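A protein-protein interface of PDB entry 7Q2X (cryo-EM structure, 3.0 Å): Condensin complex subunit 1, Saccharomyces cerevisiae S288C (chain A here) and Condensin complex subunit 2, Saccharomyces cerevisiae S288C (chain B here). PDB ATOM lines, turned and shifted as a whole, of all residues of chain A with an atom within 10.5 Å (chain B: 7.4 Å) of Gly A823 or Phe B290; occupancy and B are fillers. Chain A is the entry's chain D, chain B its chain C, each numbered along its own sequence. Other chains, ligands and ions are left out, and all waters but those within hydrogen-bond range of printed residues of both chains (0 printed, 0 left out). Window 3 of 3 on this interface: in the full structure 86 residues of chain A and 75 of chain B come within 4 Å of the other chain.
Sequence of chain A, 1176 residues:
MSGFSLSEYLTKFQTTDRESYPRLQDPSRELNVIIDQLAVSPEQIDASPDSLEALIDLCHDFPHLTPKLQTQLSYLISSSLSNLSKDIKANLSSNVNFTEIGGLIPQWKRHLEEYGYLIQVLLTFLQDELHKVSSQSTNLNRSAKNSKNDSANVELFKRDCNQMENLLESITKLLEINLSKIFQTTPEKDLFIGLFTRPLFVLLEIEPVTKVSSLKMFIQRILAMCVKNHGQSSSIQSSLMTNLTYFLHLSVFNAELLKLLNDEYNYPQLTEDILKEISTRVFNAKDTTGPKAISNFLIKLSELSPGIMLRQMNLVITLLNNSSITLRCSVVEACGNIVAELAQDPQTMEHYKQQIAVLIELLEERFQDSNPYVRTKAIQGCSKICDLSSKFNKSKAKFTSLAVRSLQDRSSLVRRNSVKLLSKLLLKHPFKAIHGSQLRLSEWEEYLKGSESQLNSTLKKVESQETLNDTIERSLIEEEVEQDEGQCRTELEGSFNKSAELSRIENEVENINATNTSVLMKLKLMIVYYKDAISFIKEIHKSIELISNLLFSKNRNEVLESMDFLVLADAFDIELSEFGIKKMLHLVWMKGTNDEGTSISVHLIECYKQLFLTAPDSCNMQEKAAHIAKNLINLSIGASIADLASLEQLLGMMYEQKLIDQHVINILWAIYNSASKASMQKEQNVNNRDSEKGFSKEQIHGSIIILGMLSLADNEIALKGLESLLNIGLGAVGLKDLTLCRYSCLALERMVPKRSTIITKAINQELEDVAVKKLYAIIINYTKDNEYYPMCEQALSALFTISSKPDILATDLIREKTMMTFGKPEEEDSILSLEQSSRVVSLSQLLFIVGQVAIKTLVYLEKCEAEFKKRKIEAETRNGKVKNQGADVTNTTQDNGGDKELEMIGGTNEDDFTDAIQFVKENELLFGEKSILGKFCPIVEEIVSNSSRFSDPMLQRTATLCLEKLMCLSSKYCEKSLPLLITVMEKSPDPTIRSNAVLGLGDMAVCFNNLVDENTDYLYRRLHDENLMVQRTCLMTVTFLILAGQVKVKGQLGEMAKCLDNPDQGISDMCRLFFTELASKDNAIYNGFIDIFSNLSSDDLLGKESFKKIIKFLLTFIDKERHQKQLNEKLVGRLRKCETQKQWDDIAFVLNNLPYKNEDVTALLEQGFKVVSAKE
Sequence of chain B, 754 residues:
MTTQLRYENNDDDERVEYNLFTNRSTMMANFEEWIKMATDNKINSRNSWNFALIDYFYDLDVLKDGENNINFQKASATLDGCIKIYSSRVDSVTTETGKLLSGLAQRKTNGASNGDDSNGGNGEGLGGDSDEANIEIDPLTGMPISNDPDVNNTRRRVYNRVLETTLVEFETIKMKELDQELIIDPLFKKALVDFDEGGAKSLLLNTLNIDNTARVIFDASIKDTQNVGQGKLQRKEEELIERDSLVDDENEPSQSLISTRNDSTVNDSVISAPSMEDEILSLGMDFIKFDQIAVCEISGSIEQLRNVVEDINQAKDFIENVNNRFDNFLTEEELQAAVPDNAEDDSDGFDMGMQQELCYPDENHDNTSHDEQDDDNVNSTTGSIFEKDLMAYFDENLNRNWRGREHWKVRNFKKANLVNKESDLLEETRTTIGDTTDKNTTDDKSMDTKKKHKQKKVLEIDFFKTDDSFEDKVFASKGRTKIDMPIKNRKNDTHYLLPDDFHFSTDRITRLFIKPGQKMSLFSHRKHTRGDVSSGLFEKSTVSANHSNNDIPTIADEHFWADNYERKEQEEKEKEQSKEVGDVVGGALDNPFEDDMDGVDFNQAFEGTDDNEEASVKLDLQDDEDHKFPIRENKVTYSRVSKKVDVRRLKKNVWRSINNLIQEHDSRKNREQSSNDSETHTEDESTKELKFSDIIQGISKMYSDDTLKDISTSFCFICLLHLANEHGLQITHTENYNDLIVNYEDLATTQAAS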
ATOM      1  N   ILE A 814      -0.946 -25.387  -3.148  1.00  0.00           N
ATOM      2  CA  ILE A 814      -0.112 -25.753  -4.289  1.00  0.00           C
ATOM      3  C   ILE A 814      -0.901 -26.608  -5.272  1.00  0.00           C
ATOM      4  O   ILE A 814      -0.815 -26.417  -6.489  1.00  0.00           O
ATOM      5  CB  ILE A 814       1.170 -26.464  -3.817  1.00  0.00           C
ATOM      6  CG1 ILE A 814       2.030 -25.509  -2.987  1.00  0.00           C
ATOM      7  CG2 ILE A 814       1.956 -26.975  -5.009  1.00  0.00           C
ATOM      8  CD1 ILE A 814       3.443 -25.999  -2.753  1.00  0.00           C
ATOM      9  N   ARG A 815      -1.695 -27.553  -4.759  1.00  0.00           N
ATOM     10  CA  ARG A 815      -2.514 -28.391  -5.629  1.00  0.00           C
ATOM     11  C   ARG A 815      -3.491 -27.550  -6.437  1.00  0.00           C
ATOM     12  O   ARG A 815      -3.634 -27.740  -7.648  1.00  0.00           O
ATOM     13  CB  ARG A 815      -3.278 -29.428  -4.807  1.00  0.00           C
ATOM     14  CG  ARG A 815      -2.439 -30.524  -4.185  1.00  0.00           C
ATOM     15  CD  ARG A 815      -3.272 -31.276  -3.163  1.00  0.00           C
ATOM     16  NE  ARG A 815      -2.557 -32.389  -2.555  1.00  0.00           N
ATOM     17  CZ  ARG A 815      -2.862 -32.913  -1.376  1.00  0.00           C
ATOM     18  NH1 ARG A 815      -3.860 -32.441  -0.647  1.00  0.00           N
ATOM     19  NH2 ARG A 815      -2.152 -33.939  -0.919  1.00  0.00           N
ATOM     20  N   GLU A 816      -4.182 -26.617  -5.778  1.00  0.00           N
ATOM     21  CA  GLU A 816      -5.169 -25.803  -6.481  1.00  0.00           C
ATOM     22  C   GLU A 816      -4.510 -24.923  -7.536  1.00  0.00           C
ATOM     23  O   GLU A 816      -4.990 -24.838  -8.676  1.00  0.00           O
ATOM     24  CB  GLU A 816      -5.954 -24.955  -5.480  1.00  0.00           C
ATOM     25  CG  GLU A 816      -7.159 -24.252  -6.077  1.00  0.00           C
ATOM     26  CD  GLU A 816      -8.179 -23.853  -5.029  1.00  0.00           C
ATOM     27  OE1 GLU A 816      -8.073 -24.334  -3.882  1.00  0.00           O
ATOM     28  OE2 GLU A 816      -9.086 -23.057  -5.352  1.00  0.00           O
ATOM     29  N   LYS A 817      -3.395 -24.277  -7.182  1.00  0.00           N
ATOM     30  CA  LYS A 817      -2.687 -23.449  -8.153  1.00  0.00           C
ATOM     31  C   LYS A 817      -2.165 -24.288  -9.311  1.00  0.00           C
ATOM     32  O   LYS A 817      -2.057 -23.802 -10.443  1.00  0.00           O
ATOM     33  CB  LYS A 817      -1.544 -22.699  -7.469  1.00  0.00           C
ATOM     34  CG  LYS A 817      -1.069 -21.470  -8.226  1.00  0.00           C
ATOM     35  CD  LYS A 817      -2.006 -20.292  -8.007  1.00  0.00           C
ATOM     36  CE  LYS A 817      -2.153 -19.461  -9.271  1.00  0.00           C
ATOM     37  NZ  LYS A 817      -2.961 -18.233  -9.034  1.00  0.00           N
ATOM     38  N   THR A 818      -1.834 -25.554  -9.047  1.00  0.00           N
ATOM     39  CA  THR A 818      -1.435 -26.457 -10.120  1.00  0.00           C
ATOM     40  C   THR A 818      -2.619 -26.815 -11.012  1.00  0.00           C
ATOM     41  O   THR A 818      -2.459 -26.966 -12.226  1.00  0.00           O
ATOM     42  CB  THR A 818      -0.806 -27.720  -9.535  1.00  0.00           C
ATOM     43  OG1 THR A 818       0.208 -27.358  -8.590  1.00  0.00           O
ATOM     44  CG2 THR A 818      -0.188 -28.561 -10.635  1.00  0.00           C
ATOM     45  N   MET A 819      -3.806 -26.978 -10.425  1.00  0.00           N
ATOM     46  CA  MET A 819      -4.990 -27.250 -11.238  1.00  0.00           C
ATOM     47  C   MET A 819      -5.338 -26.075 -12.142  1.00  0.00           C
ATOM     48  O   MET A 819      -5.729 -26.285 -13.295  1.00  0.00           O
ATOM     49  CB  MET A 819      -6.195 -27.608 -10.364  1.00  0.00           C
ATOM     50  CG  MET A 819      -5.933 -28.663  -9.309  1.00  0.00           C
ATOM     51  SD  MET A 819      -6.095 -30.340  -9.950  1.00  0.00           S
ATOM     52  CE  MET A 819      -4.879 -31.201  -8.956  1.00  0.00           C
ATOM     53  N   MET A 820      -5.214 -24.840 -11.645  1.00  0.00           N
ATOM     54  CA  MET A 820      -5.487 -23.691 -12.507  1.00  0.00           C
ATOM     55  C   MET A 820      -4.509 -23.625 -13.675  1.00  0.00           C
ATOM     56  O   MET A 820      -4.899 -23.300 -14.802  1.00  0.00           O
ATOM     57  CB  MET A 820      -5.454 -22.391 -11.704  1.00  0.00           C
ATOM     58  CG  MET A 820      -6.096 -22.489 -10.341  1.00  0.00           C
ATOM     59  SD  MET A 820      -6.696 -20.896  -9.757  1.00  0.00           S
ATOM     60  CE  MET A 820      -7.452 -21.385  -8.213  1.00  0.00           C
ATOM     61  N   THR A 821      -3.241 -23.931 -13.428  1.00  0.00           N
ATOM     62  CA  THR A 821      -2.228 -23.931 -14.470  1.00  0.00           C
ATOM     63  C   THR A 821      -2.246 -25.270 -15.213  1.00  0.00           C
ATOM     64  O   THR A 821      -2.734 -26.283 -14.710  1.00  0.00           O
ATOM     65  CB  THR A 821      -0.852 -23.651 -13.856  1.00  0.00           C
ATOM     66  OG1 THR A 821      -0.930 -22.478 -13.039  1.00  0.00           O
ATOM     67  CG2 THR A 821       0.198 -23.410 -14.933  1.00  0.00           C
ATOM     68  N   PHE A 822      -1.743 -25.257 -16.449  1.00  0.00           N
ATOM     69  CA  PHE A 822      -1.529 -26.467 -17.244  1.00  0.00           C
ATOM     70  C   PHE A 822      -2.824 -27.217 -17.543  1.00  0.00           C
ATOM     71  O   PHE A 822      -2.788 -28.396 -17.910  1.00  0.00           O
ATOM     72  CB  PHE A 822      -0.530 -27.409 -16.560  1.00  0.00           C
ATOM     73  CG  PHE A 822       0.780 -26.762 -16.216  1.00  0.00           C
ATOM     74  CD1 PHE A 822       1.436 -25.961 -17.134  1.00  0.00           C
ATOM     75  CD2 PHE A 822       1.354 -26.954 -14.970  1.00  0.00           C
ATOM     76  CE1 PHE A 822       2.642 -25.366 -16.817  1.00  0.00           C
ATOM     77  CE2 PHE A 822       2.560 -26.361 -14.649  1.00  0.00           C
ATOM     78  CZ  PHE A 822       3.204 -25.566 -15.573  1.00  0.00           C
ATOM     79  N   GLY A 823      -3.971 -26.568 -17.399  1.00  0.00           N
ATOM     80  CA  GLY A 823      -5.235 -27.232 -17.658  1.00  0.00           C
ATOM     81  C   GLY A 823      -6.377 -26.241 -17.625  1.00  0.00           C
ATOM     82  O   GLY A 823      -6.252 -25.127 -17.105  1.00  0.00           O
ATOM     83  N   LYS A 824      -7.501 -26.674 -18.195  1.00  0.00           N
ATOM     84  CA  LYS A 824      -8.703 -25.853 -18.240  1.00  0.00           C
ATOM     85  C   LYS A 824      -9.639 -26.253 -17.107  1.00  0.00           C
ATOM     86  O   LYS A 824     -10.088 -27.406 -17.070  1.00  0.00           O
ATOM     87  CB  LYS A 824      -9.411 -26.006 -19.576  1.00  0.00           C
ATOM     88  CG  LYS A 824     -10.475 -24.952 -19.839  1.00  0.00           C
ATOM     89  CD  LYS A 824     -11.003 -25.040 -21.263  1.00  0.00           C
ATOM     90  CE  LYS A 824     -11.953 -23.894 -21.573  1.00  0.00           C
ATOM     91  NZ  LYS A 824     -13.214 -23.986 -20.786  1.00  0.00           N
ATOM     92  N   PRO A 825      -9.961 -25.349 -16.171  1.00  0.00           N
ATOM     93  CA  PRO A 825     -10.847 -25.654 -15.043  1.00  0.00           C
ATOM     94  C   PRO A 825     -12.300 -25.843 -15.469  1.00  0.00           C
ATOM     95  O   PRO A 825     -12.653 -25.458 -16.584  1.00  0.00           O
ATOM     96  CB  PRO A 825     -10.701 -24.426 -14.142  1.00  0.00           C
ATOM     97  CG  PRO A 825     -10.337 -23.324 -15.073  1.00  0.00           C
ATOM     98  CD  PRO A 825      -9.493 -23.951 -16.145  1.00  0.00           C
ATOM     99  N   SER A 837      -6.932 -14.803 -19.149  1.00  0.00           N
ATOM    100  CA  SER A 837      -5.891 -14.836 -18.128  1.00  0.00           C
ATOM    101  C   SER A 837      -4.582 -15.373 -18.697  1.00  0.00           C
ATOM    102  O   SER A 837      -4.561 -16.420 -19.344  1.00  0.00           O
ATOM    103  CB  SER A 837      -6.336 -15.684 -16.935  1.00  0.00           C
ATOM    104  OG  SER A 837      -6.468 -17.047 -17.299  1.00  0.00           O
ATOM    105  N   SER A 838      -3.491 -14.652 -18.452  1.00  0.00           N
ATOM    106  CA  SER A 838      -2.186 -15.058 -18.952  1.00  0.00           C
ATOM    107  C   SER A 838      -1.636 -16.196 -18.103  1.00  0.00           C
ATOM    108  O   SER A 838      -1.532 -16.077 -16.879  1.00  0.00           O
ATOM    109  CB  SER A 838      -1.220 -13.873 -18.944  1.00  0.00           C
ATOM    110  OG  SER A 838       0.062 -14.259 -19.410  1.00  0.00           O
ATOM    111  N   ARG A 839      -1.284 -17.303 -18.759  1.00  0.00           N
ATOM    112  CA  ARG A 839      -0.828 -18.483 -18.036  1.00  0.00           C
ATOM    113  C   ARG A 839       0.596 -18.334 -17.518  1.00  0.00           C
ATOM    114  O   ARG A 839       0.969 -19.019 -16.560  1.00  0.00           O
ATOM    115  CB  ARG A 839      -0.935 -19.714 -18.935  1.00  0.00           C
ATOM    116  CG  ARG A 839      -1.058 -21.023 -18.180  1.00  0.00           C
ATOM    117  CD  ARG A 839      -1.379 -22.155 -19.131  1.00  0.00           C
ATOM    118  NE  ARG A 839      -2.729 -22.035 -19.670  1.00  0.00           N
ATOM    119  CZ  ARG A 839      -3.740 -22.832 -19.353  1.00  0.00           C
ATOM    120  NH1 ARG A 839      -3.597 -23.817 -18.482  1.00  0.00           N
ATOM    121  NH2 ARG A 839      -4.925 -22.633 -19.923  1.00  0.00           N
ATOM    122  N   SER A 842       0.330 -17.002 -14.063  1.00  0.00           N
ATOM    123  CA  SER A 842      -0.088 -18.070 -13.159  1.00  0.00           C
ATOM    124  C   SER A 842       1.075 -18.995 -12.824  1.00  0.00           C
ATOM    125  O   SER A 842       1.246 -19.397 -11.666  1.00  0.00           O
ATOM    126  CB  SER A 842      -1.242 -18.859 -13.775  1.00  0.00           C
ATOM    127  OG  SER A 842      -2.387 -18.042 -13.942  1.00  0.00           O
ATOM    128  N   LEU A 843       1.886 -19.346 -13.825  1.00  0.00           N
ATOM    129  CA  LEU A 843       3.042 -20.203 -13.575  1.00  0.00           C
ATOM    130  C   LEU A 843       4.048 -19.519 -12.656  1.00  0.00           C
ATOM    131  O   LEU A 843       4.616 -20.157 -11.762  1.00  0.00           O
ATOM    132  CB  LEU A 843       3.700 -20.594 -14.898  1.00  0.00           C
ATOM    133  CG  LEU A 843       4.957 -21.464 -14.809  1.00  0.00           C
ATOM    134  CD1 LEU A 843       4.699 -22.701 -13.963  1.00  0.00           C
ATOM    135  CD2 LEU A 843       5.442 -21.849 -16.198  1.00  0.00           C
ATOM    136  N   LEU A 846       2.697 -19.609  -9.166  1.00  0.00           N
ATOM    137  CA  LEU A 846       2.820 -20.957  -8.622  1.00  0.00           C
ATOM    138  C   LEU A 846       4.252 -21.253  -8.188  1.00  0.00           C
ATOM    139  O   LEU A 846       4.475 -21.829  -7.117  1.00  0.00           O
ATOM    140  CB  LEU A 846       2.344 -21.977  -9.657  1.00  0.00           C
ATOM    141  CG  LEU A 846       2.505 -23.465  -9.343  1.00  0.00           C
ATOM    142  CD1 LEU A 846       1.912 -23.805  -7.985  1.00  0.00           C
ATOM    143  CD2 LEU A 846       1.854 -24.295 -10.437  1.00  0.00           C
ATOM    144  N   ILE A 932       5.679 -33.074  -3.847  1.00  0.00           N
ATOM    145  CA  ILE A 932       5.295 -32.047  -4.805  1.00  0.00           C
ATOM    146  C   ILE A 932       6.496 -31.239  -5.280  1.00  0.00           C
ATOM    147  O   ILE A 932       6.623 -30.958  -6.472  1.00  0.00           O
ATOM    148  CB  ILE A 932       4.212 -31.131  -4.197  1.00  0.00           C
ATOM    149  CG1 ILE A 932       2.888 -31.883  -4.061  1.00  0.00           C
ATOM    150  CG2 ILE A 932       4.027 -29.887  -5.043  1.00  0.00           C
ATOM    151  CD1 ILE A 932       1.847 -31.142  -3.251  1.00  0.00           C
ATOM    152  N   LYS A 935       8.423 -32.893  -7.883  1.00  0.00           N
ATOM    153  CA  LYS A 935       7.747 -32.795  -9.172  1.00  0.00           C
ATOM    154  C   LYS A 935       7.979 -31.438  -9.823  1.00  0.00           C
ATOM    155  O   LYS A 935       8.049 -31.346 -11.054  1.00  0.00           O
ATOM    156  CB  LYS A 935       6.250 -33.051  -9.002  1.00  0.00           C
ATOM    157  CG  LYS A 935       5.906 -34.462  -8.556  1.00  0.00           C
ATOM    158  CD  LYS A 935       4.401 -34.663  -8.480  1.00  0.00           C
ATOM    159  CE  LYS A 935       4.053 -36.102  -8.136  1.00  0.00           C
ATOM    160  NZ  LYS A 935       4.401 -36.436  -6.728  1.00  0.00           N
ATOM    161  N   ILE A 939      10.486 -28.850 -13.798  1.00  0.00           N
ATOM    162  CA  ILE A 939       9.863 -27.710 -14.467  1.00  0.00           C
ATOM    163  C   ILE A 939      10.732 -26.469 -14.312  1.00  0.00           C
ATOM    164  O   ILE A 939      11.005 -25.747 -15.280  1.00  0.00           O
ATOM    165  CB  ILE A 939       8.443 -27.478 -13.918  1.00  0.00           C
ATOM    166  CG1 ILE A 939       7.508 -28.605 -14.361  1.00  0.00           C
ATOM    167  CG2 ILE A 939       7.909 -26.126 -14.363  1.00  0.00           C
ATOM    168  CD1 ILE A 939       6.213 -28.662 -13.583  1.00  0.00           C
ATOM    169  N   LEU B 281       1.542 -25.287 -22.021  1.00  0.00           N
ATOM    170  CA  LEU B 281       0.735 -26.505 -21.960  1.00  0.00           C
ATOM    171  C   LEU B 281       1.562 -27.742 -22.286  1.00  0.00           C
ATOM    172  O   LEU B 281       1.380 -28.794 -21.664  1.00  0.00           O
ATOM    173  CB  LEU B 281      -0.475 -26.405 -22.893  1.00  0.00           C
ATOM    174  CG  LEU B 281      -1.749 -25.692 -22.417  1.00  0.00           C
ATOM    175  CD1 LEU B 281      -2.354 -26.444 -21.240  1.00  0.00           C
ATOM    176  CD2 LEU B 281      -1.527 -24.239 -22.048  1.00  0.00           C
ATOM    177  N   GLY B 284       3.691 -28.541 -19.228  1.00  0.00           N
ATOM    178  CA  GLY B 284       2.852 -29.102 -18.183  1.00  0.00           C
ATOM    179  C   GLY B 284       2.441 -30.532 -18.472  1.00  0.00           C
ATOM    180  O   GLY B 284       2.492 -31.392 -17.593  1.00  0.00           O
ATOM    181  N   MET B 285       2.046 -30.811 -19.715  1.00  0.00           N
ATOM    182  CA  MET B 285       1.692 -32.176 -20.085  1.00  0.00           C
ATOM    183  C   MET B 285       2.893 -33.104 -19.965  1.00  0.00           C
ATOM    184  O   MET B 285       2.751 -34.270 -19.578  1.00  0.00           O
ATOM    185  CB  MET B 285       1.130 -32.205 -21.506  1.00  0.00           C
ATOM    186  CG  MET B 285       0.612 -33.564 -21.939  1.00  0.00           C
ATOM    187  SD  MET B 285      -0.803 -34.098 -20.959  1.00  0.00           S
ATOM    188  CE  MET B 285      -2.073 -33.000 -21.583  1.00  0.00           C
ATOM    189  N   ILE B 288       4.189 -33.013 -15.632  1.00  0.00           N
ATOM    190  CA  ILE B 288       3.294 -33.119 -14.482  1.00  0.00           C
ATOM    191  C   ILE B 288       1.969 -33.685 -14.970  1.00  0.00           C
ATOM    192  O   ILE B 288       1.577 -33.481 -16.122  1.00  0.00           O
ATOM    193  CB  ILE B 288       3.119 -31.759 -13.754  1.00  0.00           C
ATOM    194  CG1 ILE B 288       2.401 -31.952 -12.419  1.00  0.00           C
ATOM    195  CG2 ILE B 288       2.344 -30.773 -14.604  1.00  0.00           C
ATOM    196  CD1 ILE B 288       2.478 -30.749 -11.515  1.00  0.00           C
ATOM    197  N   LYS B 289       1.287 -34.417 -14.092  1.00  0.00           N
ATOM    198  CA  LYS B 289       0.011 -35.037 -14.413  1.00  0.00           C
ATOM    199  C   LYS B 289      -1.026 -34.639 -13.374  1.00  0.00           C
ATOM    200  O   LYS B 289      -0.689 -34.304 -12.235  1.00  0.00           O
ATOM    201  CB  LYS B 289       0.127 -36.568 -14.477  1.00  0.00           C
ATOM    202  CG  LYS B 289       1.498 -37.076 -14.895  1.00  0.00           C
ATOM    203  CD  LYS B 289       1.404 -38.437 -15.562  1.00  0.00           C
ATOM    204  CE  LYS B 289       2.783 -38.976 -15.907  1.00  0.00           C
ATOM    205  NZ  LYS B 289       2.708 -40.222 -16.717  1.00  0.00           N
ATOM    206  N   PHE B 290      -2.296 -34.673 -13.784  1.00  0.00           N
ATOM    207  CA  PHE B 290      -3.378 -34.318 -12.870  1.00  0.00           C
ATOM    208  C   PHE B 290      -3.447 -35.281 -11.692  1.00  0.00           C
ATOM    209  O   PHE B 290      -3.638 -34.859 -10.546  1.00  0.00           O
ATOM    210  CB  PHE B 290      -4.709 -34.288 -13.620  1.00  0.00           C
ATOM    211  CG  PHE B 290      -4.869 -33.100 -14.526  1.00  0.00           C
ATOM    212  CD1 PHE B 290      -4.151 -31.937 -14.300  1.00  0.00           C
ATOM    213  CD2 PHE B 290      -5.740 -33.146 -15.602  1.00  0.00           C
ATOM    214  CE1 PHE B 290      -4.298 -30.843 -15.131  1.00  0.00           C
ATOM    215  CE2 PHE B 290      -5.890 -32.054 -16.438  1.00  0.00           C
ATOM    216  CZ  PHE B 290      -5.169 -30.902 -16.201  1.00  0.00           C
ATOM    217  N   ASP B 291      -3.294 -36.577 -11.952  1.00  0.00           N
ATOM    218  CA  ASP B 291      -3.307 -37.562 -10.885  1.00  0.00           C
ATOM    219  C   ASP B 291      -1.995 -37.525 -10.101  1.00  0.00           C
ATOM    220  O   ASP B 291      -1.018 -36.882 -10.498  1.00  0.00           O
ATOM    221  CB  ASP B 291      -3.576 -38.961 -11.447  1.00  0.00           C
ATOM    222  CG  ASP B 291      -2.493 -39.436 -12.406  1.00  0.00           C
ATOM    223  OD1 ASP B 291      -1.542 -38.677 -12.684  1.00  0.00           O
ATOM    224  OD2 ASP B 291      -2.598 -40.584 -12.888  1.00  0.00           O
ATOM    225  N   GLN B 292      -1.990 -38.225  -8.966  1.00  0.00           N
ATOM    226  CA  GLN B 292      -0.839 -38.280  -8.063  1.00  0.00           C
ATOM    227  C   GLN B 292      -0.437 -36.890  -7.574  1.00  0.00           C
ATOM    228  O   GLN B 292       0.744 -36.618  -7.344  1.00  0.00           O
ATOM    229  CB  GLN B 292       0.355 -38.983  -8.718  1.00  0.00           C
ATOM    230  CG  GLN B 292       0.155 -40.474  -8.930  1.00  0.00           C
ATOM    231  CD  GLN B 292       0.988 -41.017 -10.074  1.00  0.00           C
ATOM    232  OE1 GLN B 292       0.635 -40.859 -11.244  1.00  0.00           O
ATOM    233  NE2 GLN B 292       2.100 -41.662  -9.743  1.00  0.00           N
ATOM    234  N   ILE B 293      -1.418 -36.001  -7.418  1.00  0.00           N
ATOM    235  CA  ILE B 293      -1.202 -34.651  -6.910  1.00  0.00           C
ATOM    236  C   ILE B 293      -2.059 -34.379  -5.679  1.00  0.00           C
ATOM    237  O   ILE B 293      -1.571 -33.862  -4.669  1.00  0.00           O
ATOM    238  CB  ILE B 293      -1.462 -33.591  -8.003  1.00  0.00           C
ATOM    239  CG1 ILE B 293      -0.370 -33.647  -9.073  1.00  0.00           C
ATOM    240  CG2 ILE B 293      -1.545 -32.198  -7.396  1.00  0.00           C
ATOM    241  CD1 ILE B 293       0.958 -33.080  -8.624  1.00  0.00           C
ATOM    242  N   ALA B 294      -3.344 -34.732  -5.742  1.00  0.00           N
ATOM    243  CA  ALA B 294      -4.256 -34.501  -4.629  1.00  0.00           C
ATOM    244  C   ALA B 294      -4.013 -35.441  -3.456  1.00  0.00           C
ATOM    245  O   ALA B 294      -4.606 -35.237  -2.391  1.00  0.00           O
ATOM    246  CB  ALA B 294      -5.705 -34.631  -5.101  1.00  0.00           C
ATOM    247  N   VAL B 295      -3.171 -36.460  -3.621  1.00  0.00           N
ATOM    248  CA  VAL B 295      -2.903 -37.418  -2.555  1.00  0.00           C
ATOM    249  C   VAL B 295      -1.422 -37.393  -2.202  1.00  0.00           C
ATOM    250  O   VAL B 295      -0.853 -38.413  -1.796  1.00  0.00           O
ATOM    251  CB  VAL B 295      -3.349 -38.835  -2.958  1.00  0.00           C
ATOM    252  CG1 VAL B 295      -4.867 -38.937  -2.939  1.00  0.00           C
ATOM    253  CG2 VAL B 295      -2.802 -39.192  -4.331  1.00  0.00           C
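The backbone carbonyl oxygen of Ile B293 is in hydrogen-bond range of the guanidinium group of Arg A815, at 2.8 Å. O of Ala B294 sits close to NH2 of Arg A815, 3.1 Å away.
Of the 21 printed residues of chain A, 7 touch a printed residue of chain B. Hydrophobic or aromatic side chains of chain A that line the printed part of chain B: Met A819 and Phe A822. Among the printed residues, 13 pairs touch across the chains.
The side-chain carboxylate (OD1) of Asp B291 lies close to the side-chain amide oxygen (OE1) of Gln B292. The backbone carbonyl oxygen (O) of Ile A814 sits at hydrogen-bond distance from the side-chain hydroxyl (OG1) of Thr A818, 2.5 Å away. The guanidinium group of Arg A839 sits at hydrogen-bond distance from the backbone carbonyl oxygen of Gly A823 (3.3 Å).
Of chain B, only Phe B290 comes within 4 Å of Gly A823. No residue of chain A comes within 4 Å of Asp B291. Ile B293 touches just these residues of chain A: Arg A815, Met A819 and Lys A935. Of the printed residues of chain B, Lys A935 touches Gln B292 (3.4 Å) and Ile B293 (3.8 Å). Of the printed residues of chain A, Leu B281 touches Phe A822 (3.8 Å) and Arg A839 (3.5 Å). Of the printed residues of chain A, Ile B288 touches Thr A818 (3.6 Å) and Phe A822 (3.96 Å). Printed residues of chain B within 4 Å of Phe A822: Leu B281 (3.8 Å), Gly B284 (3.6 Å), Ile B288 (3.96 Å) and Phe B290 (3.9 Å). The nearest printed residue of chain A that does not touch Gln B292 is Ile A932 (6.1 Å).
Among the printed residues, pairs that only touch across the chains: Arg A815 with Val B295 (3.8 Å), Thr A818 with Ile B288 (3.6 Å), Met A819 with Ile B293 (3.8 Å), Phe A822 with Leu B281 (3.8 Å), Phe A822 with Gly B284 (3.6 Å), Phe A822 with Ile B288 (3.96 Å), Phe A822 with Phe B290 (3.9 Å), Gly A823 with Phe B290 (3.9 Å), Arg A839 with Leu B281 (3.5 Å), Lys A935 with Gln B292 (3.4 Å) and Lys A935 with Ile B293 (3.8 Å).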
